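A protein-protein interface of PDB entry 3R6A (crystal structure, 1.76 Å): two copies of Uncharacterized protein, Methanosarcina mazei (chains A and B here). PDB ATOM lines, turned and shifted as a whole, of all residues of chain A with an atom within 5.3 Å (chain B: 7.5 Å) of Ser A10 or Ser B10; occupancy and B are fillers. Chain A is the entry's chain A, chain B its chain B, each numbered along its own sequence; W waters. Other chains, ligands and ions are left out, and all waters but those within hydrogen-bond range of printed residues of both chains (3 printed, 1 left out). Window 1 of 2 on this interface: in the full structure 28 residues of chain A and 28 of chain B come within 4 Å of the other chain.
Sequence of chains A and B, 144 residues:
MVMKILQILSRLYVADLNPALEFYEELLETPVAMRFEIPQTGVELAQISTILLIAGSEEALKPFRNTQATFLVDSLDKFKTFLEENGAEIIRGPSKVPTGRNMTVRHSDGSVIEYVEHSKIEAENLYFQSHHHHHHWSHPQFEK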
ATOM      1  N   ILE A   8      29.671  20.348 -35.332  1.00  0.00           N
ATOM      2  CA  ILE A   8      29.443  20.641 -33.929  1.00  0.00           C
ATOM      3  C   ILE A   8      28.152  21.447 -33.912  1.00  0.00           C
ATOM      4  O   ILE A   8      28.101  22.567 -34.416  1.00  0.00           O
ATOM      5  CB  ILE A   8      30.596  21.444 -33.330  1.00  0.00           C
ATOM      6  CG1 ILE A   8      31.874  20.600 -33.406  1.00  0.00           C
ATOM      7  CG2 ILE A   8      30.276  21.806 -31.888  1.00  0.00           C
ATOM      8  CD1 ILE A   8      33.123  21.282 -32.852  1.00  0.00           C
ATOM      9  N   LEU A   9      27.110  20.856 -33.342  1.00  0.00           N
ATOM     10  CA  LEU A   9      25.792  21.479 -33.304  1.00  0.00           C
ATOM     11  C   LEU A   9      25.458  22.124 -31.971  1.00  0.00           C
ATOM     12  O   LEU A   9      25.571  21.497 -30.916  1.00  0.00           O
ATOM     13  CB  LEU A   9      24.736  20.426 -33.648  1.00  0.00           C
ATOM     14  CG  LEU A   9      25.064  19.636 -34.919  1.00  0.00           C
ATOM     15  CD1 LEU A   9      24.063  18.507 -35.104  1.00  0.00           C
ATOM     16  CD2 LEU A   9      25.056  20.566 -36.127  1.00  0.00           C
ATOM     17  N   SER A  10      25.043  23.384 -32.031  1.00  0.00           N
ATOM     18  CA  SER A  10      24.669  24.122 -30.840  1.00  0.00           C
ATOM     19  C   SER A  10      23.208  23.796 -30.588  1.00  0.00           C
ATOM     20  O   SER A  10      22.449  23.597 -31.531  1.00  0.00           O
ATOM     21  CB  SER A  10      24.858  25.617 -31.074  1.00  0.00           C
ATOM     22  OG  SER A  10      26.199  25.873 -31.444  1.00  0.00           O
ATOM     23  N   ARG A  11      22.820  23.749 -29.322  1.00  0.00           N
ATOM     24  CA  ARG A  11      21.459  23.385 -28.967  1.00  0.00           C
ATOM     25  C   ARG A  11      20.619  24.522 -28.398  1.00  0.00           C
ATOM     26  O   ARG A  11      21.044  25.229 -27.487  1.00  0.00           O
ATOM     27  CB  ARG A  11      21.501  22.238 -27.952  1.00  0.00           C
ATOM     28  CG  ARG A  11      22.201  20.987 -28.452  1.00  0.00           C
ATOM     29  CD  ARG A  11      22.789  20.177 -27.298  1.00  0.00           C
ATOM     30  NE  ARG A  11      21.789  19.525 -26.451  1.00  0.00           N
ATOM     31  CZ  ARG A  11      21.238  18.339 -26.698  1.00  0.00           C
ATOM     32  NH1 ARG A  11      21.574  17.647 -27.778  1.00  0.00           N
ATOM     33  NH2 ARG A  11      20.350  17.832 -25.848  1.00  0.00           N
ATOM     34  N   LEU A  12      19.419  24.683 -28.948  1.00  0.00           N
ATOM     35  CA  LEU A  12      18.485  25.697 -28.480  1.00  0.00           C
ATOM     36  C   LEU A  12      17.229  24.956 -28.043  1.00  0.00           C
ATOM     37  O   LEU A  12      16.858  23.939 -28.629  1.00  0.00           O
ATOM     38  CB  LEU A  12      18.164  26.708 -29.581  1.00  0.00           C
ATOM     39  CG  LEU A  12      19.334  27.586 -30.035  1.00  0.00           C
ATOM     40  CD1 LEU A  12      18.811  28.691 -30.957  1.00  0.00           C
ATOM     41  CD2 LEU A  12      20.029  28.192 -28.823  1.00  0.00           C
ATOM     42  N   THR A  50      23.749  24.893 -38.385  1.00  0.00           N
ATOM     43  CA  THR A  50      24.392  24.024 -37.399  1.00  0.00           C
ATOM     44  C   THR A  50      23.755  24.158 -36.016  1.00  0.00           C
ATOM     45  O   THR A  50      24.407  23.955 -34.989  1.00  0.00           O
ATOM     46  CB  THR A  50      25.926  24.275 -37.293  1.00  0.00           C
ATOM     47  OG1 THR A  50      26.183  25.647 -36.973  1.00  0.00           O
ATOM     48  CG2 THR A  50      26.612  23.918 -38.617  1.00  0.00           C
ATOM     49  N   ILE A  51      22.472  24.506 -36.005  1.00  0.00           N
ATOM     50  CA  ILE A  51      21.709  24.637 -34.769  1.00  0.00           C
ATOM     51  C   ILE A  51      20.689  23.515 -34.678  1.00  0.00           C
ATOM     52  O   ILE A  51      20.016  23.192 -35.664  1.00  0.00           O
ATOM     53  CB  ILE A  51      20.912  25.967 -34.714  1.00  0.00           C
ATOM     54  CG1 ILE A  51      21.864  27.141 -34.477  1.00  0.00           C
ATOM     55  CG2 ILE A  51      19.858  25.906 -33.604  1.00  0.00           C
ATOM     56  CD1 ILE A  51      21.208  28.492 -34.609  1.00  0.00           C
ATOM     57  N   LEU A  52      20.596  22.908 -33.501  1.00  0.00           N
ATOM     58  CA  LEU A  52      19.604  21.876 -33.251  1.00  0.00           C
ATOM     59  C   LEU A  52      18.536  22.550 -32.403  1.00  0.00           C
ATOM     60  O   LEU A  52      18.834  23.099 -31.337  1.00  0.00           O
ATOM     61  CB  LEU A  52      20.199  20.700 -32.468  1.00  0.00           C
ATOM     62  CG  LEU A  52      21.077  19.704 -33.223  1.00  0.00           C
ATOM     63  CD1 LEU A  52      21.620  18.672 -32.235  1.00  0.00           C
ATOM     64  CD2 LEU A  52      20.261  19.014 -34.321  1.00  0.00           C
ATOM     65  N   ALA A  69      26.348  20.376 -25.967  1.00  0.00           N
ATOM     66  CA  ALA A  69      26.367  20.400 -27.425  1.00  0.00           C
ATOM     67  C   ALA A  69      26.287  18.997 -27.995  1.00  0.00           C
ATOM     68  O   ALA A  69      26.415  18.012 -27.271  1.00  0.00           O
ATOM     69  CB  ALA A  69      27.646  21.075 -27.917  1.00  0.00           C
ATOM     70  N   GLN B   7      29.871  32.402 -38.340  1.00  0.00           N
ATOM     71  CA  GLN B   7      30.101  31.174 -37.586  1.00  0.00           C
ATOM     72  C   GLN B   7      29.144  31.102 -36.417  1.00  0.00           C
ATOM     73  O   GLN B   7      28.748  32.130 -35.868  1.00  0.00           O
ATOM     74  CB  GLN B   7      31.508  31.124 -36.984  1.00  0.00           C
ATOM     75  CG  GLN B   7      32.660  30.894 -37.927  1.00  0.00           C
ATOM     76  CD  GLN B   7      33.938  30.613 -37.156  1.00  0.00           C
ATOM     77  OE1 GLN B   7      34.333  31.388 -36.281  1.00  0.00           O
ATOM     78  NE2 GLN B   7      34.587  29.496 -37.471  1.00  0.00           N
ATOM     79  N   ILE B   8      28.786  29.880 -36.039  1.00  0.00           N
ATOM     80  CA  ILE B   8      27.934  29.661 -34.880  1.00  0.00           C
ATOM     81  C   ILE B   8      28.860  28.923 -33.927  1.00  0.00           C
ATOM     82  O   ILE B   8      29.310  27.812 -34.217  1.00  0.00           O
ATOM     83  CB  ILE B   8      26.713  28.794 -35.219  1.00  0.00           C
ATOM     84  CG1 ILE B   8      25.823  29.547 -36.213  1.00  0.00           C
ATOM     85  CG2 ILE B   8      25.941  28.460 -33.942  1.00  0.00           C
ATOM     86  CD1 ILE B   8      24.550  28.804 -36.613  1.00  0.00           C
ATOM     87  N   LEU B   9      29.168  29.556 -32.802  1.00  0.00           N
ATOM     88  CA  LEU B   9      30.084  28.973 -31.834  1.00  0.00           C
ATOM     89  C   LEU B   9      29.384  28.356 -30.637  1.00  0.00           C
ATOM     90  O   LEU B   9      28.553  29.001 -29.988  1.00  0.00           O
ATOM     91  CB  LEU B   9      31.069  30.049 -31.366  1.00  0.00           C
ATOM     92  CG  LEU B   9      31.801  30.761 -32.506  1.00  0.00           C
ATOM     93  CD1 LEU B   9      32.600  31.934 -31.957  1.00  0.00           C
ATOM     94  CD2 LEU B   9      32.717  29.772 -33.222  1.00  0.00           C
ATOM     95  N   SER B  10      29.722  27.100 -30.356  1.00  0.00           N
ATOM     96  CA  SER B  10      29.149  26.376 -29.221  1.00  0.00           C
ATOM     97  C   SER B  10      30.003  26.681 -27.997  1.00  0.00           C
ATOM     98  O   SER B  10      31.229  26.709 -28.078  1.00  0.00           O
ATOM     99  CB  SER B  10      29.145  24.876 -29.501  1.00  0.00           C
ATOM    100  OG  SER B  10      28.398  24.603 -30.674  1.00  0.00           O
ATOM    101  N   ARG B  11      29.346  26.879 -26.862  1.00  0.00           N
ATOM    102  CA  ARG B  11      30.028  27.245 -25.630  1.00  0.00           C
ATOM    103  C   ARG B  11      30.179  26.126 -24.611  1.00  0.00           C
ATOM    104  O   ARG B  11      29.219  25.427 -24.301  1.00  0.00           O
ATOM    105  CB  ARG B  11      29.277  28.406 -24.977  1.00  0.00           C
ATOM    106  CG  ARG B  11      29.168  29.649 -25.854  1.00  0.00           C
ATOM    107  CD  ARG B  11      27.957  30.492 -25.458  1.00  0.00           C
ATOM    108  NE  ARG B  11      28.076  31.108 -24.131  1.00  0.00           N
ATOM    109  CZ  ARG B  11      28.649  32.286 -23.898  1.00  0.00           C
ATOM    110  NH1 ARG B  11      29.168  32.987 -24.898  1.00  0.00           N
ATOM    111  NH2 ARG B  11      28.680  32.781 -22.665  1.00  0.00           N
ATOM    112  N   LEU B  12      31.395  25.969 -24.100  1.00  0.00           N
ATOM    113  CA  LEU B  12      31.681  24.978 -23.074  1.00  0.00           C
ATOM    114  C   LEU B  12      32.291  25.755 -21.911  1.00  0.00           C
ATOM    115  O   LEU B  12      33.037  26.719 -22.115  1.00  0.00           O
ATOM    116  CB  LEU B  12      32.663  23.911 -23.578  1.00  0.00           C
ATOM    117  CG  LEU B  12      32.185  23.009 -24.719  1.00  0.00           C
ATOM    118  CD1 LEU B  12      33.208  21.907 -24.960  1.00  0.00           C
ATOM    119  CD2 LEU B  12      30.832  22.398 -24.376  1.00  0.00           C
ATOM    120  N   TYR B  13      31.964  25.331 -20.696  1.00  0.00           N
ATOM    121  CA  TYR B  13      32.428  25.988 -19.482  1.00  0.00           C
ATOM    122  C   TYR B  13      33.293  25.044 -18.669  1.00  0.00           C
ATOM    123  O   TYR B  13      32.860  23.952 -18.303  1.00  0.00           O
ATOM    124  CB  TYR B  13      31.214  26.427 -18.672  1.00  0.00           C
ATOM    125  CG  TYR B  13      30.195  27.135 -19.525  1.00  0.00           C
ATOM    126  CD1 TYR B  13      30.243  28.517 -19.702  1.00  0.00           C
ATOM    127  CD2 TYR B  13      29.213  26.416 -20.210  1.00  0.00           C
ATOM    128  CE1 TYR B  13      29.340  29.165 -20.543  1.00  0.00           C
ATOM    129  CE2 TYR B  13      28.310  27.053 -21.051  1.00  0.00           C
ATOM    130  CZ  TYR B  13      28.379  28.427 -21.213  1.00  0.00           C
ATOM    131  OH  TYR B  13      27.489  29.059 -22.047  1.00  0.00           O
ATOM    132  N   ALA B  46      38.888  31.005 -24.897  1.00  0.00           N
ATOM    133  CA  ALA B  46      39.687  30.384 -25.950  1.00  0.00           C
ATOM    134  C   ALA B  46      38.753  29.822 -27.014  1.00  0.00           C
ATOM    135  O   ALA B  46      37.597  29.505 -26.730  1.00  0.00           O
ATOM    136  CB  ALA B  46      40.541  29.260 -25.376  1.00  0.00           C
ATOM    137  N   GLN B  47      39.237  29.720 -28.246  1.00  0.00           N
ATOM    138  CA  GLN B  47      38.421  29.134 -29.302  1.00  0.00           C
ATOM    139  C   GLN B  47      39.217  28.058 -30.007  1.00  0.00           C
ATOM    140  O   GLN B  47      40.362  28.283 -30.400  1.00  0.00           O
ATOM    141  CB  GLN B  47      37.980  30.172 -30.339  1.00  0.00           C
ATOM    142  CG  GLN B  47      37.031  29.567 -31.394  1.00  0.00           C
ATOM    143  CD  GLN B  47      36.630  30.546 -32.482  1.00  0.00           C
ATOM    144  OE1 GLN B  47      36.518  31.743 -32.242  1.00  0.00           O
ATOM    145  NE2 GLN B  47      36.394  30.030 -33.688  1.00  0.00           N
ATOM    146  N   ILE B  48      38.620  26.881 -30.145  1.00  0.00           N
ATOM    147  CA  ILE B  48      39.257  25.776 -30.849  1.00  0.00           C
ATOM    148  C   ILE B  48      38.170  25.256 -31.783  1.00  0.00           C
ATOM    149  O   ILE B  48      37.069  24.923 -31.334  1.00  0.00           O
ATOM    150  CB  ILE B  48      39.746  24.694 -29.864  1.00  0.00           C
ATOM    151  CG1 ILE B  48      40.400  23.550 -30.642  1.00  0.00           C
ATOM    152  CG2 ILE B  48      38.602  24.216 -28.994  1.00  0.00           C
ATOM    153  CD1 ILE B  48      41.276  22.666 -29.789  1.00  0.00           C
ATOM    154  N   THR B  50      35.068  25.354 -33.794  1.00  0.00           N
ATOM    155  CA  THR B  50      33.926  26.249 -33.555  1.00  0.00           C
ATOM    156  C   THR B  50      33.428  26.181 -32.115  1.00  0.00           C
ATOM    157  O   THR B  50      32.264  26.462 -31.824  1.00  0.00           O
ATOM    158  CB  THR B  50      32.737  25.959 -34.514  1.00  0.00           C
ATOM    159  OG1 THR B  50      32.294  24.606 -34.364  1.00  0.00           O
ATOM    160  CG2 THR B  50      33.165  26.189 -35.953  1.00  0.00           C
ATOM    161  N   ILE B  51      34.327  25.808 -31.214  1.00  0.00           N
ATOM    162  CA  ILE B  51      33.996  25.724 -29.802  1.00  0.00           C
ATOM    163  C   ILE B  51      34.639  26.878 -29.042  1.00  0.00           C
ATOM    164  O   ILE B  51      35.814  27.164 -29.226  1.00  0.00           O
ATOM    165  CB  ILE B  51      34.519  24.420 -29.182  1.00  0.00           C
ATOM    166  CG1 ILE B  51      33.785  23.224 -29.788  1.00  0.00           C
ATOM    167  CG2 ILE B  51      34.325  24.445 -27.670  1.00  0.00           C
ATOM    168  CD1 ILE B  51      34.293  21.903 -29.294  1.00  0.00           C
ATOM    169  N   LEU B  52      33.857  27.536 -28.194  1.00  0.00           N
ATOM    170  CA  LEU B  52      34.369  28.618 -27.371  1.00  0.00           C
ATOM    171  C   LEU B  52      34.496  28.034 -25.978  1.00  0.00           C
ATOM    172  O   LEU B  52      33.499  27.606 -25.391  1.00  0.00           O
ATOM    173  CB  LEU B  52      33.396  29.806 -27.325  1.00  0.00           C
ATOM    174  CG  LEU B  52      33.330  30.770 -28.509  1.00  0.00           C
ATOM    175  CD1 LEU B  52      32.255  31.824 -28.246  1.00  0.00           C
ATOM    176  CD2 LEU B  52      34.684  31.441 -28.700  1.00  0.00           C
ATOM    177  N   LEU B  53      35.722  27.987 -25.463  1.00  0.00           N
ATOM    178  CA  LEU B  53      35.975  27.477 -24.123  1.00  0.00           C
ATOM    179  C   LEU B  53      36.059  28.663 -23.169  1.00  0.00           C
ATOM    180  O   LEU B  53      36.907  29.545 -23.333  1.00  0.00           O
ATOM    181  CB  LEU B  53      37.290  26.692 -24.079  1.00  0.00           C
ATOM    182  CG  LEU B  53      37.334  25.328 -24.757  1.00  0.00           C
ATOM    183  CD1 LEU B  53      38.764  24.786 -24.708  1.00  0.00           C
ATOM    184  CD2 LEU B  53      36.376  24.365 -24.054  1.00  0.00           C
ATOM    185  N   ILE B  54      35.166  28.683 -22.182  1.00  0.00           N
ATOM    186  CA  ILE B  54      35.118  29.752 -21.190  1.00  0.00           C
ATOM    187  C   ILE B  54      35.541  29.135 -19.859  1.00  0.00           C
ATOM    188  O   ILE B  54      34.884  28.220 -19.366  1.00  0.00           O
ATOM    189  CB  ILE B  54      33.687  30.311 -21.086  1.00  0.00           C
ATOM    190  CG1 ILE B  54      33.222  30.761 -22.475  1.00  0.00           C
ATOM    191  CG2 ILE B  54      33.642  31.469 -20.095  1.00  0.00           C
ATOM    192  CD1 ILE B  54      31.774  31.171 -22.538  1.00  0.00           C
ATOM    193  N   GLN B  68      23.105  30.660 -24.581  1.00  0.00           N
ATOM    194  CA  GLN B  68      23.056  29.381 -25.291  1.00  0.00           C
ATOM    195  C   GLN B  68      24.178  29.172 -26.307  1.00  0.00           C
ATOM    196  O   GLN B  68      24.741  28.077 -26.413  1.00  0.00           O
ATOM    197  CB  GLN B  68      21.710  29.240 -26.012  1.00  0.00           C
ATOM    198  CG  GLN B  68      20.483  29.499 -25.141  1.00  0.00           C
ATOM    199  CD  GLN B  68      20.372  28.526 -23.995  1.00  0.00           C
ATOM    200  OE1 GLN B  68      20.385  27.311 -24.196  1.00  0.00           O
ATOM    201  NE2 GLN B  68      20.255  29.051 -22.781  1.00  0.00           N
ATOM    202  N   ALA B  69      24.493  30.216 -27.063  1.00  0.00           N
ATOM    203  CA  ALA B  69      25.525  30.127 -28.089  1.00  0.00           C
ATOM    204  C   ALA B  69      25.975  31.509 -28.521  1.00  0.00           C
ATOM    205  O   ALA B  69      25.381  32.514 -28.139  1.00  0.00           O
ATOM    206  CB  ALA B  69      24.994  29.360 -29.292  1.00  0.00           C
ATOM    207  N   THR B  70      27.033  31.546 -29.323  1.00  0.00           N
ATOM    208  CA  THR B  70      27.582  32.801 -29.818  1.00  0.00           C
ATOM    209  C   THR B  70      27.562  32.797 -31.341  1.00  0.00           C
ATOM    210  O   THR B  70      28.015  31.844 -31.979  1.00  0.00           O
ATOM    211  CB  THR B  70      29.023  32.984 -29.307  1.00  0.00           C
ATOM    212  OG1 THR B  70      28.992  33.159 -27.885  1.00  0.00           O
ATOM    213  CG2 THR B  70      29.694  34.186 -29.958  1.00  0.00           C
ATOM    214  N   PHE B  71      27.006  33.858 -31.916  1.00  0.00           N
ATOM    215  CA  PHE B  71      26.931  33.993 -33.363  1.00  0.00           C
ATOM    216  C   PHE B  71      27.918  35.055 -33.807  1.00  0.00           C
ATOM    217  O   PHE B  71      27.791  36.215 -33.421  1.00  0.00           O
ATOM    218  CB  PHE B  71      25.538  34.452 -33.820  1.00  0.00           C
ATOM    219  CG  PHE B  71      24.440  33.438 -33.634  1.00  0.00           C
ATOM    220  CD1 PHE B  71      24.681  32.197 -33.054  1.00  0.00           C
ATOM    221  CD2 PHE B  71      23.142  33.746 -34.044  1.00  0.00           C
ATOM    222  CE1 PHE B  71      23.644  31.281 -32.881  1.00  0.00           C
ATOM    223  CE2 PHE B  71      22.101  32.838 -33.875  1.00  0.00           C
ATOM    224  CZ  PHE B  71      22.356  31.601 -33.292  1.00  0.00           C
ATOM    225  N   ILE B 113      21.293  34.663 -26.907  1.00  0.00           N
ATOM    226  CA  ILE B 113      22.413  34.524 -27.826  1.00  0.00           C
ATOM    227  C   ILE B 113      23.343  35.728 -27.806  1.00  0.00           C
ATOM    228  O   ILE B 113      22.891  36.875 -27.730  1.00  0.00           O
ATOM    229  CB  ILE B 113      21.899  34.354 -29.274  1.00  0.00           C
ATOM    230  CG1 ILE B 113      20.994  33.120 -29.369  1.00  0.00           C
ATOM    231  CG2 ILE B 113      23.084  34.283 -30.246  1.00  0.00           C
ATOM    232  CD1 ILE B 113      21.702  31.793 -29.149  1.00  0.00           C
HETATM  233  O   HOH W   1      22.891  25.522 -25.647  1.00  0.00           O
HETATM  234  O   HOH W   2      29.783  25.182 -33.185  1.00  0.00           O
HETATM  235  O   HOH W   3      29.197  25.457 -36.103  1.00  0.00           O
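The side-chain hydroxyl of Ser A10 is in hydrogen-bond range of the side-chain hydroxyl of Ser B10 (2.7 Å).
O of Thr B50 is in hydrogen-bond range of N of Ser B10 (3.0 Å). The backbone carbonyl oxygen of Ser A10 sits at hydrogen-bond distance from the backbone NH of Leu A52 (2.8 Å). N of Leu A12 lies within hydrogen-bond range of O of Leu A52, 2.9 Å away. The backbone carbonyl oxygen (O) of Thr A50 is in hydrogen-bond range of the backbone NH (N) of Ser A10, at 3.1 Å. The backbone carbonyl oxygen of Ser B10 sits at hydrogen-bond distance from the backbone NH of Leu B52, at 2.8 Å.
Among the printed residues, pairs that only touch across the chains: Ile A8 with Ser B10, Ile A8 with Thr B50, Ile A8 with Ile B51, Ser A10 with Ile B8, Arg A11 with Gln B68, Leu A12 with Gln B68, Leu A12 with Ile B113, Thr A50 with Ile B8, Ile A51 with Ile B8 and Ile A51 with Phe B71.
Of the printed residues of chain B, Ile A8 touches Ser B10 (3.6 Å), Thr B50 (3.7 Å) and Ile B51 (3.7 Å). Ser A10 touches just these residues of chain B: Ile B8 (3.6 Å) and Ser B10 (2.7 Å). Printed residues of chain B within 4 Å of Arg A11: Gln B68 (3.9 Å). Of chain A, only Ile A8 (3.6 Å) and Ser A10 (2.7 Å) come within 4 Å of Ser B10. Ile B48 touches none of the printed residues of chain A. The nearest printed residue of chain A that does not touch Ile B8 is Ile A8 (5.4 Å).
Of the 9 printed residues of chain A, 6 touch a printed residue of chain B. Printed residues of chain A that touch a printed residue of chain B: Ile A8, Ser A10, Arg A11, Leu A12, Thr A50 and Ile A51. Of the 20 printed residues of chain B, 7 touch a printed residue of chain A. Among the printed residues, 11 pairs touch across the chains. Among the printed residues, no Asp or Glu carboxylate lies within 4 Å of a Lys or Arg side-chain nitrogen of the other chain.
Ile A8 touches Ser B10, and with the chains exchanged Ser A10 touches Ile B8. Ile A8 touches Thr B50, and with the chains exchanged Thr A50 touches Ile B8. Ile A8 touches Ile B51, and with the chains exchanged Ile A51 touches Ile B8. Ser B10 touches its own counterpart, Ser A10.
Water W1 bridges O of Arg A11 and O of Gln B68. Water W2 lies within hydrogen-bond range of OG1 of Thr B50, O of Ile B8, OG of Ser B10 and O of Ile A8. Water W3 lies within hydrogen-bond range of O of Ile B8 (3.0 Å) and OG1 of Thr A50 (3.1 Å).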
